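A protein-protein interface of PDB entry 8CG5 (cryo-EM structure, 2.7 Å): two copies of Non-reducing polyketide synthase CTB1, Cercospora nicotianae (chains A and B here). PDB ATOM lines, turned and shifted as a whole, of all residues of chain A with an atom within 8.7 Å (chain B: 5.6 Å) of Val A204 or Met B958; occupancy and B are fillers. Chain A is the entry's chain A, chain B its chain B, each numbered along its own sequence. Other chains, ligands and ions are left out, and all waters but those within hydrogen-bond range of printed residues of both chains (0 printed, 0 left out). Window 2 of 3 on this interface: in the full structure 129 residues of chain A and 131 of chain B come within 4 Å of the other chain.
Gln B953 touches Ile A158 (OE1 to CD1, 3.9 Å). SG of Cys A161 touches CD1 of Ile B954, 3.2 Å away. N of Ser B1026 touches O of Cys A161 (3.6 Å). CD2 of Leu A162 touches OG of Ser B1026 (3.9 Å). Val A204 touches Gly B957. CG of Met B958 touches CG2 of Val A204, at 3.7 Å.
Of the printed residues of chain B, Ile A158 touches Gln B953. Of the printed residues of chain B, Leu A162 touches Ser B1026. Ala A251 touches none of the printed residues of chain B. Glu B956 touches none of the printed residues of chain A. Gly B957 touches one residue of chain A. Met B958 touches just one residue of chain A: Val A204. No residue of chain A comes within 4 Å of Ser B959. Of the printed residues of chain A, Ser B1026 touches Cys A161 (3.6 Å) and Leu A162 (3.9 Å). The nearest residue of chain B that does not touch Val A204 is Ile B954 (4.1 Å).
Of the 11 printed residues of chain B, 5 touch a printed residue of chain A. Printed residues of chain B that touch a printed residue of chain A: Gln B953, Ile B954, Gly B957, Met B958 and Ser B1026. Hydrophobic or aromatic side chains of chain B that line the printed part of chain A: Ile B954 and Met B958. Printed residues of chain A that touch a printed residue of chain B: Ile A158, Cys A161, Leu A162 and Val A204. Hydrophobic or aromatic side chains of chain A within 4 Å of the printed part of chain B: Ile A158, Leu A162 and Val A204. Among the printed residues, 6 pairs touch across the chains.
No position is printed for both chains. Of the 6 pairs that touch across the chains among the printed residues, none has its exchanged pair printed and touching as well.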
ATOM      1  N   ILE A 158     -29.256  22.121  -9.033  1.00  0.00           N
ATOM      2  CA  ILE A 158     -28.912  21.195  -7.957  1.00  0.00           C
ATOM      3  C   ILE A 158     -29.367  19.784  -8.311  1.00  0.00           C
ATOM      4  O   ILE A 158     -28.625  18.809  -8.137  1.00  0.00           O
ATOM      5  CB  ILE A 158     -29.513  21.664  -6.620  1.00  0.00           C
ATOM      6  CG1 ILE A 158     -28.777  22.910  -6.125  1.00  0.00           C
ATOM      7  CG2 ILE A 158     -29.443  20.547  -5.587  1.00  0.00           C
ATOM      8  CD1 ILE A 158     -27.531  22.614  -5.319  1.00  0.00           C
ATOM      9  N   CYS A 161     -27.134  18.226 -10.983  1.00  0.00           N
ATOM     10  CA  CYS A 161     -25.884  17.786 -10.375  1.00  0.00           C
ATOM     11  C   CYS A 161     -26.086  16.531  -9.540  1.00  0.00           C
ATOM     12  O   CYS A 161     -25.153  15.738  -9.383  1.00  0.00           O
ATOM     13  CB  CYS A 161     -25.294  18.899  -9.515  1.00  0.00           C
ATOM     14  SG  CYS A 161     -23.771  18.438  -8.669  1.00  0.00           S
ATOM     15  N   LEU A 162     -27.284  16.339  -8.988  1.00  0.00           N
ATOM     16  CA  LEU A 162     -27.543  15.158  -8.170  1.00  0.00           C
ATOM     17  C   LEU A 162     -27.697  13.897  -9.012  1.00  0.00           C
ATOM     18  O   LEU A 162     -27.168  12.841  -8.651  1.00  0.00           O
ATOM     19  CB  LEU A 162     -28.798  15.376  -7.325  1.00  0.00           C
ATOM     20  CG  LEU A 162     -28.610  15.753  -5.857  1.00  0.00           C
ATOM     21  CD1 LEU A 162     -29.924  15.619  -5.121  1.00  0.00           C
ATOM     22  CD2 LEU A 162     -27.571  14.874  -5.205  1.00  0.00           C
ATOM     23  N   ALA A 163     -28.422  13.980 -10.124  1.00  0.00           N
ATOM     24  CA  ALA A 163     -28.644  12.821 -10.973  1.00  0.00           C
ATOM     25  C   ALA A 163     -28.712  13.278 -12.420  1.00  0.00           C
ATOM     26  O   ALA A 163     -29.003  14.439 -12.712  1.00  0.00           O
ATOM     27  CB  ALA A 163     -29.924  12.076 -10.586  1.00  0.00           C
ATOM     28  N   TRP A 176     -39.760  14.106  -9.691  1.00  0.00           N
ATOM     29  CA  TRP A 176     -38.919  14.014  -8.509  1.00  0.00           C
ATOM     30  C   TRP A 176     -39.705  13.775  -7.229  1.00  0.00           C
ATOM     31  O   TRP A 176     -39.098  13.708  -6.157  1.00  0.00           O
ATOM     32  CB  TRP A 176     -38.090  15.290  -8.362  1.00  0.00           C
ATOM     33  CG  TRP A 176     -36.799  15.254  -9.111  1.00  0.00           C
ATOM     34  CD1 TRP A 176     -36.636  15.292 -10.462  1.00  0.00           C
ATOM     35  CD2 TRP A 176     -35.486  15.183  -8.549  1.00  0.00           C
ATOM     36  NE1 TRP A 176     -35.302  15.243 -10.777  1.00  0.00           N
ATOM     37  CE2 TRP A 176     -34.575  15.178  -9.619  1.00  0.00           C
ATOM     38  CE3 TRP A 176     -34.993  15.122  -7.244  1.00  0.00           C
ATOM     39  CZ2 TRP A 176     -33.202  15.113  -9.427  1.00  0.00           C
ATOM     40  CZ3 TRP A 176     -33.630  15.059  -7.055  1.00  0.00           C
ATOM     41  CH2 TRP A 176     -32.750  15.054  -8.140  1.00  0.00           C
ATOM     42  N   THR A 196     -33.056   4.142   4.523  1.00  0.00           N
ATOM     43  CA  THR A 196     -31.743   4.747   4.329  1.00  0.00           C
ATOM     44  C   THR A 196     -30.707   4.202   5.301  1.00  0.00           C
ATOM     45  O   THR A 196     -29.507   4.325   5.036  1.00  0.00           O
ATOM     46  CB  THR A 196     -31.825   6.268   4.465  1.00  0.00           C
ATOM     47  OG1 THR A 196     -30.567   6.846   4.101  1.00  0.00           O
ATOM     48  CG2 THR A 196     -32.164   6.670   5.889  1.00  0.00           C
ATOM     49  N   LEU A 201     -26.623   4.926   1.491  1.00  0.00           N
ATOM     50  CA  LEU A 201     -26.889   5.964   0.509  1.00  0.00           C
ATOM     51  C   LEU A 201     -26.157   7.233   0.913  1.00  0.00           C
ATOM     52  O   LEU A 201     -25.933   7.488   2.099  1.00  0.00           O
ATOM     53  CB  LEU A 201     -28.389   6.251   0.380  1.00  0.00           C
ATOM     54  CG  LEU A 201     -29.147   5.421  -0.653  1.00  0.00           C
ATOM     55  CD1 LEU A 201     -30.597   5.252  -0.239  1.00  0.00           C
ATOM     56  CD2 LEU A 201     -29.055   6.068  -2.021  1.00  0.00           C
ATOM     57  N   ALA A 202     -25.787   8.028  -0.086  1.00  0.00           N
ATOM     58  CA  ALA A 202     -25.165   9.312   0.190  1.00  0.00           C
ATOM     59  C   ALA A 202     -26.130  10.203   0.960  1.00  0.00           C
ATOM     60  O   ALA A 202     -27.310  10.306   0.619  1.00  0.00           O
ATOM     61  CB  ALA A 202     -24.744   9.991  -1.113  1.00  0.00           C
ATOM     62  N   SER A 203     -25.617  10.861   2.001  1.00  0.00           N
ATOM     63  CA  SER A 203     -26.471  11.708   2.825  1.00  0.00           C
ATOM     64  C   SER A 203     -27.160  12.780   1.994  1.00  0.00           C
ATOM     65  O   SER A 203     -28.229  13.269   2.372  1.00  0.00           O
ATOM     66  CB  SER A 203     -25.648  12.353   3.938  1.00  0.00           C
ATOM     67  OG  SER A 203     -26.486  13.013   4.870  1.00  0.00           O
ATOM     68  N   VAL A 204     -26.565  13.155   0.859  1.00  0.00           N
ATOM     69  CA  VAL A 204     -27.125  14.191   0.002  1.00  0.00           C
ATOM     70  C   VAL A 204     -28.132  13.633  -0.996  1.00  0.00           C
ATOM     71  O   VAL A 204     -28.787  14.412  -1.702  1.00  0.00           O
ATOM     72  CB  VAL A 204     -25.952  14.928  -0.687  1.00  0.00           C
ATOM     73  CG1 VAL A 204     -26.363  15.571  -1.997  1.00  0.00           C
ATOM     74  CG2 VAL A 204     -25.372  15.973   0.251  1.00  0.00           C
ATOM     75  N   SER A 205     -28.311  12.310  -1.049  1.00  0.00           N
ATOM     76  CA  SER A 205     -29.167  11.693  -2.056  1.00  0.00           C
ATOM     77  C   SER A 205     -30.255  10.802  -1.466  1.00  0.00           C
ATOM     78  O   SER A 205     -30.890  10.051  -2.213  1.00  0.00           O
ATOM     79  CB  SER A 205     -28.320  10.877  -3.036  1.00  0.00           C
ATOM     80  OG  SER A 205     -29.048   9.768  -3.524  1.00  0.00           O
ATOM     81  N   VAL A 206     -30.495  10.863  -0.160  1.00  0.00           N
ATOM     82  CA  VAL A 206     -31.507  10.027   0.483  1.00  0.00           C
ATOM     83  C   VAL A 206     -32.897  10.540   0.128  1.00  0.00           C
ATOM     84  O   VAL A 206     -33.041  11.702  -0.275  1.00  0.00           O
ATOM     85  CB  VAL A 206     -31.317   9.994   2.006  1.00  0.00           C
ATOM     86  CG1 VAL A 206     -29.969   9.403   2.357  1.00  0.00           C
ATOM     87  CG2 VAL A 206     -31.466  11.390   2.597  1.00  0.00           C
ATOM     88  N   PRO A 207     -33.938   9.720   0.250  1.00  0.00           N
ATOM     89  CA  PRO A 207     -35.300  10.219   0.044  1.00  0.00           C
ATOM     90  C   PRO A 207     -35.829  10.955   1.263  1.00  0.00           C
ATOM     91  O   PRO A 207     -35.517  10.627   2.409  1.00  0.00           O
ATOM     92  CB  PRO A 207     -36.103   8.940  -0.220  1.00  0.00           C
ATOM     93  CG  PRO A 207     -35.366   7.888   0.511  1.00  0.00           C
ATOM     94  CD  PRO A 207     -33.912   8.262   0.457  1.00  0.00           C
ATOM     95  N   TYR A 208     -36.650  11.967   0.995  1.00  0.00           N
ATOM     96  CA  TYR A 208     -37.222  12.805   2.036  1.00  0.00           C
ATOM     97  C   TYR A 208     -38.673  13.106   1.695  1.00  0.00           C
ATOM     98  O   TYR A 208     -39.066  13.085   0.526  1.00  0.00           O
ATOM     99  CB  TYR A 208     -36.442  14.115   2.189  1.00  0.00           C
ATOM    100  CG  TYR A 208     -36.466  14.977   0.949  1.00  0.00           C
ATOM    101  CD1 TYR A 208     -35.699  14.654  -0.157  1.00  0.00           C
ATOM    102  CD2 TYR A 208     -37.257  16.110   0.884  1.00  0.00           C
ATOM    103  CE1 TYR A 208     -35.721  15.436  -1.288  1.00  0.00           C
ATOM    104  CE2 TYR A 208     -37.284  16.895  -0.243  1.00  0.00           C
ATOM    105  CZ  TYR A 208     -36.514  16.554  -1.326  1.00  0.00           C
ATOM    106  OH  TYR A 208     -36.539  17.337  -2.453  1.00  0.00           O
ATOM    107  N   ALA A 222     -37.212  12.376  -4.106  1.00  0.00           N
ATOM    108  CA  ALA A 222     -35.882  11.804  -4.255  1.00  0.00           C
ATOM    109  C   ALA A 222     -35.569  11.799  -5.745  1.00  0.00           C
ATOM    110  O   ALA A 222     -36.430  12.103  -6.576  1.00  0.00           O
ATOM    111  CB  ALA A 222     -35.785  10.394  -3.677  1.00  0.00           C
ATOM    112  N   ALA A 223     -34.333  11.454  -6.076  1.00  0.00           N
ATOM    113  CA  ALA A 223     -33.965  11.352  -7.477  1.00  0.00           C
ATOM    114  C   ALA A 223     -34.830  10.286  -8.146  1.00  0.00           C
ATOM    115  O   ALA A 223     -35.100   9.242  -7.540  1.00  0.00           O
ATOM    116  CB  ALA A 223     -32.485  11.004  -7.624  1.00  0.00           C
ATOM    117  N   ILE A 226     -33.908   6.709  -7.493  1.00  0.00           N
ATOM    118  CA  ILE A 226     -33.962   6.338  -6.084  1.00  0.00           C
ATOM    119  C   ILE A 226     -35.403   6.325  -5.595  1.00  0.00           C
ATOM    120  O   ILE A 226     -35.802   5.452  -4.817  1.00  0.00           O
ATOM    121  CB  ILE A 226     -33.084   7.290  -5.256  1.00  0.00           C
ATOM    122  CG1 ILE A 226     -31.684   7.350  -5.871  1.00  0.00           C
ATOM    123  CG2 ILE A 226     -33.029   6.836  -3.804  1.00  0.00           C
ATOM    124  CD1 ILE A 226     -30.596   7.740  -4.913  1.00  0.00           C
ATOM    125  N   PRO A 248     -35.820  19.010  -7.358  1.00  0.00           N
ATOM    126  CA  PRO A 248     -35.942  18.895  -5.901  1.00  0.00           C
ATOM    127  C   PRO A 248     -36.348  20.212  -5.261  1.00  0.00           C
ATOM    128  O   PRO A 248     -35.856  21.283  -5.622  1.00  0.00           O
ATOM    129  CB  PRO A 248     -34.536  18.474  -5.459  1.00  0.00           C
ATOM    130  CG  PRO A 248     -33.638  18.953  -6.527  1.00  0.00           C
ATOM    131  CD  PRO A 248     -34.418  18.958  -7.804  1.00  0.00           C
ATOM    132  N   ALA A 251     -36.044  20.938   0.440  1.00  0.00           N
ATOM    133  CA  ALA A 251     -34.974  20.080   0.936  1.00  0.00           C
ATOM    134  C   ALA A 251     -34.042  20.887   1.825  1.00  0.00           C
ATOM    135  O   ALA A 251     -33.151  21.583   1.317  1.00  0.00           O
ATOM    136  CB  ALA A 251     -34.198  19.466  -0.232  1.00  0.00           C
ATOM    137  N   HIS A 253     -31.618  19.865   3.343  1.00  0.00           N
ATOM    138  CA  HIS A 253     -30.301  19.252   3.262  1.00  0.00           C
ATOM    139  C   HIS A 253     -29.640  19.451   1.906  1.00  0.00           C
ATOM    140  O   HIS A 253     -28.557  18.904   1.677  1.00  0.00           O
ATOM    141  CB  HIS A 253     -30.400  17.755   3.568  1.00  0.00           C
ATOM    142  CG  HIS A 253     -31.370  17.025   2.696  1.00  0.00           C
ATOM    143  ND1 HIS A 253     -31.037  16.550   1.446  1.00  0.00           N
ATOM    144  CD2 HIS A 253     -32.668  16.691   2.890  1.00  0.00           C
ATOM    145  CE1 HIS A 253     -32.087  15.956   0.909  1.00  0.00           C
ATOM    146  NE2 HIS A 253     -33.089  16.027   1.765  1.00  0.00           N
ATOM    147  N   LEU A 254     -30.261  20.210   1.002  1.00  0.00           N
ATOM    148  CA  LEU A 254     -29.674  20.526  -0.289  1.00  0.00           C
ATOM    149  C   LEU A 254     -29.512  22.017  -0.532  1.00  0.00           C
ATOM    150  O   LEU A 254     -28.790  22.394  -1.460  1.00  0.00           O
ATOM    151  CB  LEU A 254     -30.523  19.941  -1.428  1.00  0.00           C
ATOM    152  CG  LEU A 254     -30.689  18.424  -1.472  1.00  0.00           C
ATOM    153  CD1 LEU A 254     -31.648  18.038  -2.581  1.00  0.00           C
ATOM    154  CD2 LEU A 254     -29.353  17.745  -1.667  1.00  0.00           C
ATOM    155  N   PHE A 255     -30.153  22.869   0.263  1.00  0.00           N
ATOM    156  CA  PHE A 255     -30.118  24.308   0.059  1.00  0.00           C
ATOM    157  C   PHE A 255     -29.770  24.999   1.367  1.00  0.00           C
ATOM    158  O   PHE A 255     -30.066  24.494   2.453  1.00  0.00           O
ATOM    159  CB  PHE A 255     -31.459  24.830  -0.458  1.00  0.00           C
ATOM    160  CG  PHE A 255     -31.915  24.173  -1.725  1.00  0.00           C
ATOM    161  CD1 PHE A 255     -31.405  24.564  -2.946  1.00  0.00           C
ATOM    162  CD2 PHE A 255     -32.861  23.166  -1.695  1.00  0.00           C
ATOM    163  CE1 PHE A 255     -31.827  23.963  -4.110  1.00  0.00           C
ATOM    164  CE2 PHE A 255     -33.284  22.562  -2.856  1.00  0.00           C
ATOM    165  CZ  PHE A 255     -32.767  22.962  -4.064  1.00  0.00           C
ATOM    166  N   GLN B 953     -20.394  23.162  -1.815  1.00  0.00           N
ATOM    167  CA  GLN B 953     -21.630  23.023  -1.053  1.00  0.00           C
ATOM    168  C   GLN B 953     -21.995  21.557  -0.880  1.00  0.00           C
ATOM    169  O   GLN B 953     -22.351  21.114   0.218  1.00  0.00           O
ATOM    170  CB  GLN B 953     -22.756  23.779  -1.754  1.00  0.00           C
ATOM    171  CG  GLN B 953     -23.725  24.467  -0.812  1.00  0.00           C
ATOM    172  CD  GLN B 953     -25.095  24.664  -1.429  1.00  0.00           C
ATOM    173  OE1 GLN B 953     -25.340  24.266  -2.568  1.00  0.00           O
ATOM    174  NE2 GLN B 953     -25.996  25.282  -0.677  1.00  0.00           N
ATOM    175  N   ILE B 954     -21.898  20.782  -1.960  1.00  0.00           N
ATOM    176  CA  ILE B 954     -22.252  19.368  -1.894  1.00  0.00           C
ATOM    177  C   ILE B 954     -21.304  18.620  -0.965  1.00  0.00           C
ATOM    178  O   ILE B 954     -21.735  17.784  -0.164  1.00  0.00           O
ATOM    179  CB  ILE B 954     -22.269  18.767  -3.308  1.00  0.00           C
ATOM    180  CG1 ILE B 954     -23.546  19.197  -4.029  1.00  0.00           C
ATOM    181  CG2 ILE B 954     -22.161  17.253  -3.246  1.00  0.00           C
ATOM    182  CD1 ILE B 954     -23.598  18.816  -5.484  1.00  0.00           C
ATOM    183  N   CYS B 955     -20.002  18.903  -1.052  1.00  0.00           N
ATOM    184  CA  CYS B 955     -19.046  18.240  -0.172  1.00  0.00           C
ATOM    185  C   CYS B 955     -19.325  18.563   1.288  1.00  0.00           C
ATOM    186  O   CYS B 955     -19.301  17.672   2.143  1.00  0.00           O
ATOM    187  CB  CYS B 955     -17.619  18.641  -0.543  1.00  0.00           C
ATOM    188  SG  CYS B 955     -17.051  18.008  -2.135  1.00  0.00           S
ATOM    189  N   GLU B 956     -19.591  19.834   1.596  1.00  0.00           N
ATOM    190  CA  GLU B 956     -19.960  20.181   2.964  1.00  0.00           C
ATOM    191  C   GLU B 956     -21.244  19.480   3.380  1.00  0.00           C
ATOM    192  O   GLU B 956     -21.432  19.179   4.563  1.00  0.00           O
ATOM    193  CB  GLU B 956     -20.112  21.694   3.103  1.00  0.00           C
ATOM    194  CG  GLU B 956     -18.826  22.470   2.881  1.00  0.00           C
ATOM    195  CD  GLU B 956     -19.064  23.953   2.672  1.00  0.00           C
ATOM    196  OE1 GLU B 956     -20.210  24.338   2.361  1.00  0.00           O
ATOM    197  OE2 GLU B 956     -18.103  24.736   2.818  1.00  0.00           O
ATOM    198  N   GLY B 957     -22.137  19.216   2.425  1.00  0.00           N
ATOM    199  CA  GLY B 957     -23.345  18.474   2.745  1.00  0.00           C
ATOM    200  C   GLY B 957     -23.059  17.047   3.174  1.00  0.00           C
ATOM    201  O   GLY B 957     -23.678  16.537   4.111  1.00  0.00           O
ATOM    202  N   MET B 958     -22.120  16.384   2.499  1.00  0.00           N
ATOM    203  CA  MET B 958     -21.789  14.995   2.775  1.00  0.00           C
ATOM    204  C   MET B 958     -20.749  14.846   3.877  1.00  0.00           C
ATOM    205  O   MET B 958     -20.142  13.778   4.005  1.00  0.00           O
ATOM    206  CB  MET B 958     -21.293  14.313   1.498  1.00  0.00           C
ATOM    207  CG  MET B 958     -22.405  13.851   0.580  1.00  0.00           C
ATOM    208  SD  MET B 958     -21.798  13.123  -0.949  1.00  0.00           S
ATOM    209  CE  MET B 958     -20.901  14.503  -1.645  1.00  0.00           C
ATOM    210  N   SER B 959     -20.531  15.889   4.675  1.00  0.00           N
ATOM    211  CA  SER B 959     -19.557  15.859   5.764  1.00  0.00           C
ATOM    212  C   SER B 959     -18.156  15.584   5.219  1.00  0.00           C
ATOM    213  O   SER B 959     -17.491  14.615   5.584  1.00  0.00           O
ATOM    214  CB  SER B 959     -19.952  14.825   6.822  1.00  0.00           C
ATOM    215  OG  SER B 959     -21.101  15.244   7.536  1.00  0.00           O
ATOM    216  N   LEU B 960     -17.722  16.465   4.327  1.00  0.00           N
ATOM    217  CA  LEU B 960     -16.397  16.390   3.738  1.00  0.00           C
ATOM    218  C   LEU B 960     -15.714  17.743   3.815  1.00  0.00           C
ATOM    219  O   LEU B 960     -16.385  18.780   3.878  1.00  0.00           O
ATOM    220  CB  LEU B 960     -16.441  15.950   2.271  1.00  0.00           C
ATOM    221  CG  LEU B 960     -16.788  14.491   2.018  1.00  0.00           C
ATOM    222  CD1 LEU B 960     -17.179  14.318   0.569  1.00  0.00           C
ATOM    223  CD2 LEU B 960     -15.614  13.600   2.378  1.00  0.00           C
ATOM    224  N   SER B1026     -22.213  14.283  -8.011  1.00  0.00           N
ATOM    225  CA  SER B1026     -22.312  13.992  -6.586  1.00  0.00           C
ATOM    226  C   SER B1026     -21.805  12.590  -6.281  1.00  0.00           C
ATOM    227  O   SER B1026     -21.126  12.376  -5.274  1.00  0.00           O
ATOM    228  CB  SER B1026     -23.754  14.152  -6.115  1.00  0.00           C
ATOM    229  OG  SER B1026     -24.281  12.912  -5.680  1.00  0.00           O
ATOM    230  N   LEU B1029     -17.949  12.679  -6.369  1.00  0.00           N
ATOM    231  CA  LEU B1029     -17.397  13.301  -5.172  1.00  0.00           C
ATOM    232  C   LEU B1029     -17.555  12.389  -3.965  1.00  0.00           C
ATOM    233  O   LEU B1029     -16.634  12.258  -3.153  1.00  0.00           O
ATOM    234  CB  LEU B1029     -18.072  14.646  -4.920  1.00  0.00           C
ATOM    235  CG  LEU B1029     -17.882  15.695  -6.015  1.00  0.00           C
ATOM    236  CD1 LEU B1029     -18.741  16.912  -5.741  1.00  0.00           C
ATOM    237  CD2 LEU B1029     -16.424  16.091  -6.132  1.00  0.00           C
ATOM    238  N   TYR B1030     -18.717  11.749  -3.832  1.00  0.00           N
ATOM    239  CA  TYR B1030     -18.949  10.858  -2.703  1.00  0.00           C
ATOM    240  C   TYR B1030     -17.953   9.709  -2.704  1.00  0.00           C
ATOM    241  O   TYR B1030     -17.345   9.398  -1.676  1.00  0.00           O
ATOM    242  CB  TYR B1030     -20.381  10.329  -2.752  1.00  0.00           C
ATOM    243  CG  TYR B1030     -20.758   9.459  -1.578  1.00  0.00           C
ATOM    244  CD1 TYR B1030     -20.669   9.934  -0.279  1.00  0.00           C
ATOM    245  CD2 TYR B1030     -21.209   8.162  -1.769  1.00  0.00           C
ATOM    246  CE1 TYR B1030     -21.015   9.143   0.794  1.00  0.00           C
ATOM    247  CE2 TYR B1030     -21.555   7.364  -0.703  1.00  0.00           C
ATOM    248  CZ  TYR B1030     -21.457   7.859   0.575  1.00  0.00           C
ATOM    249  OH  TYR B1030     -21.802   7.066   1.644  1.00  0.00           O
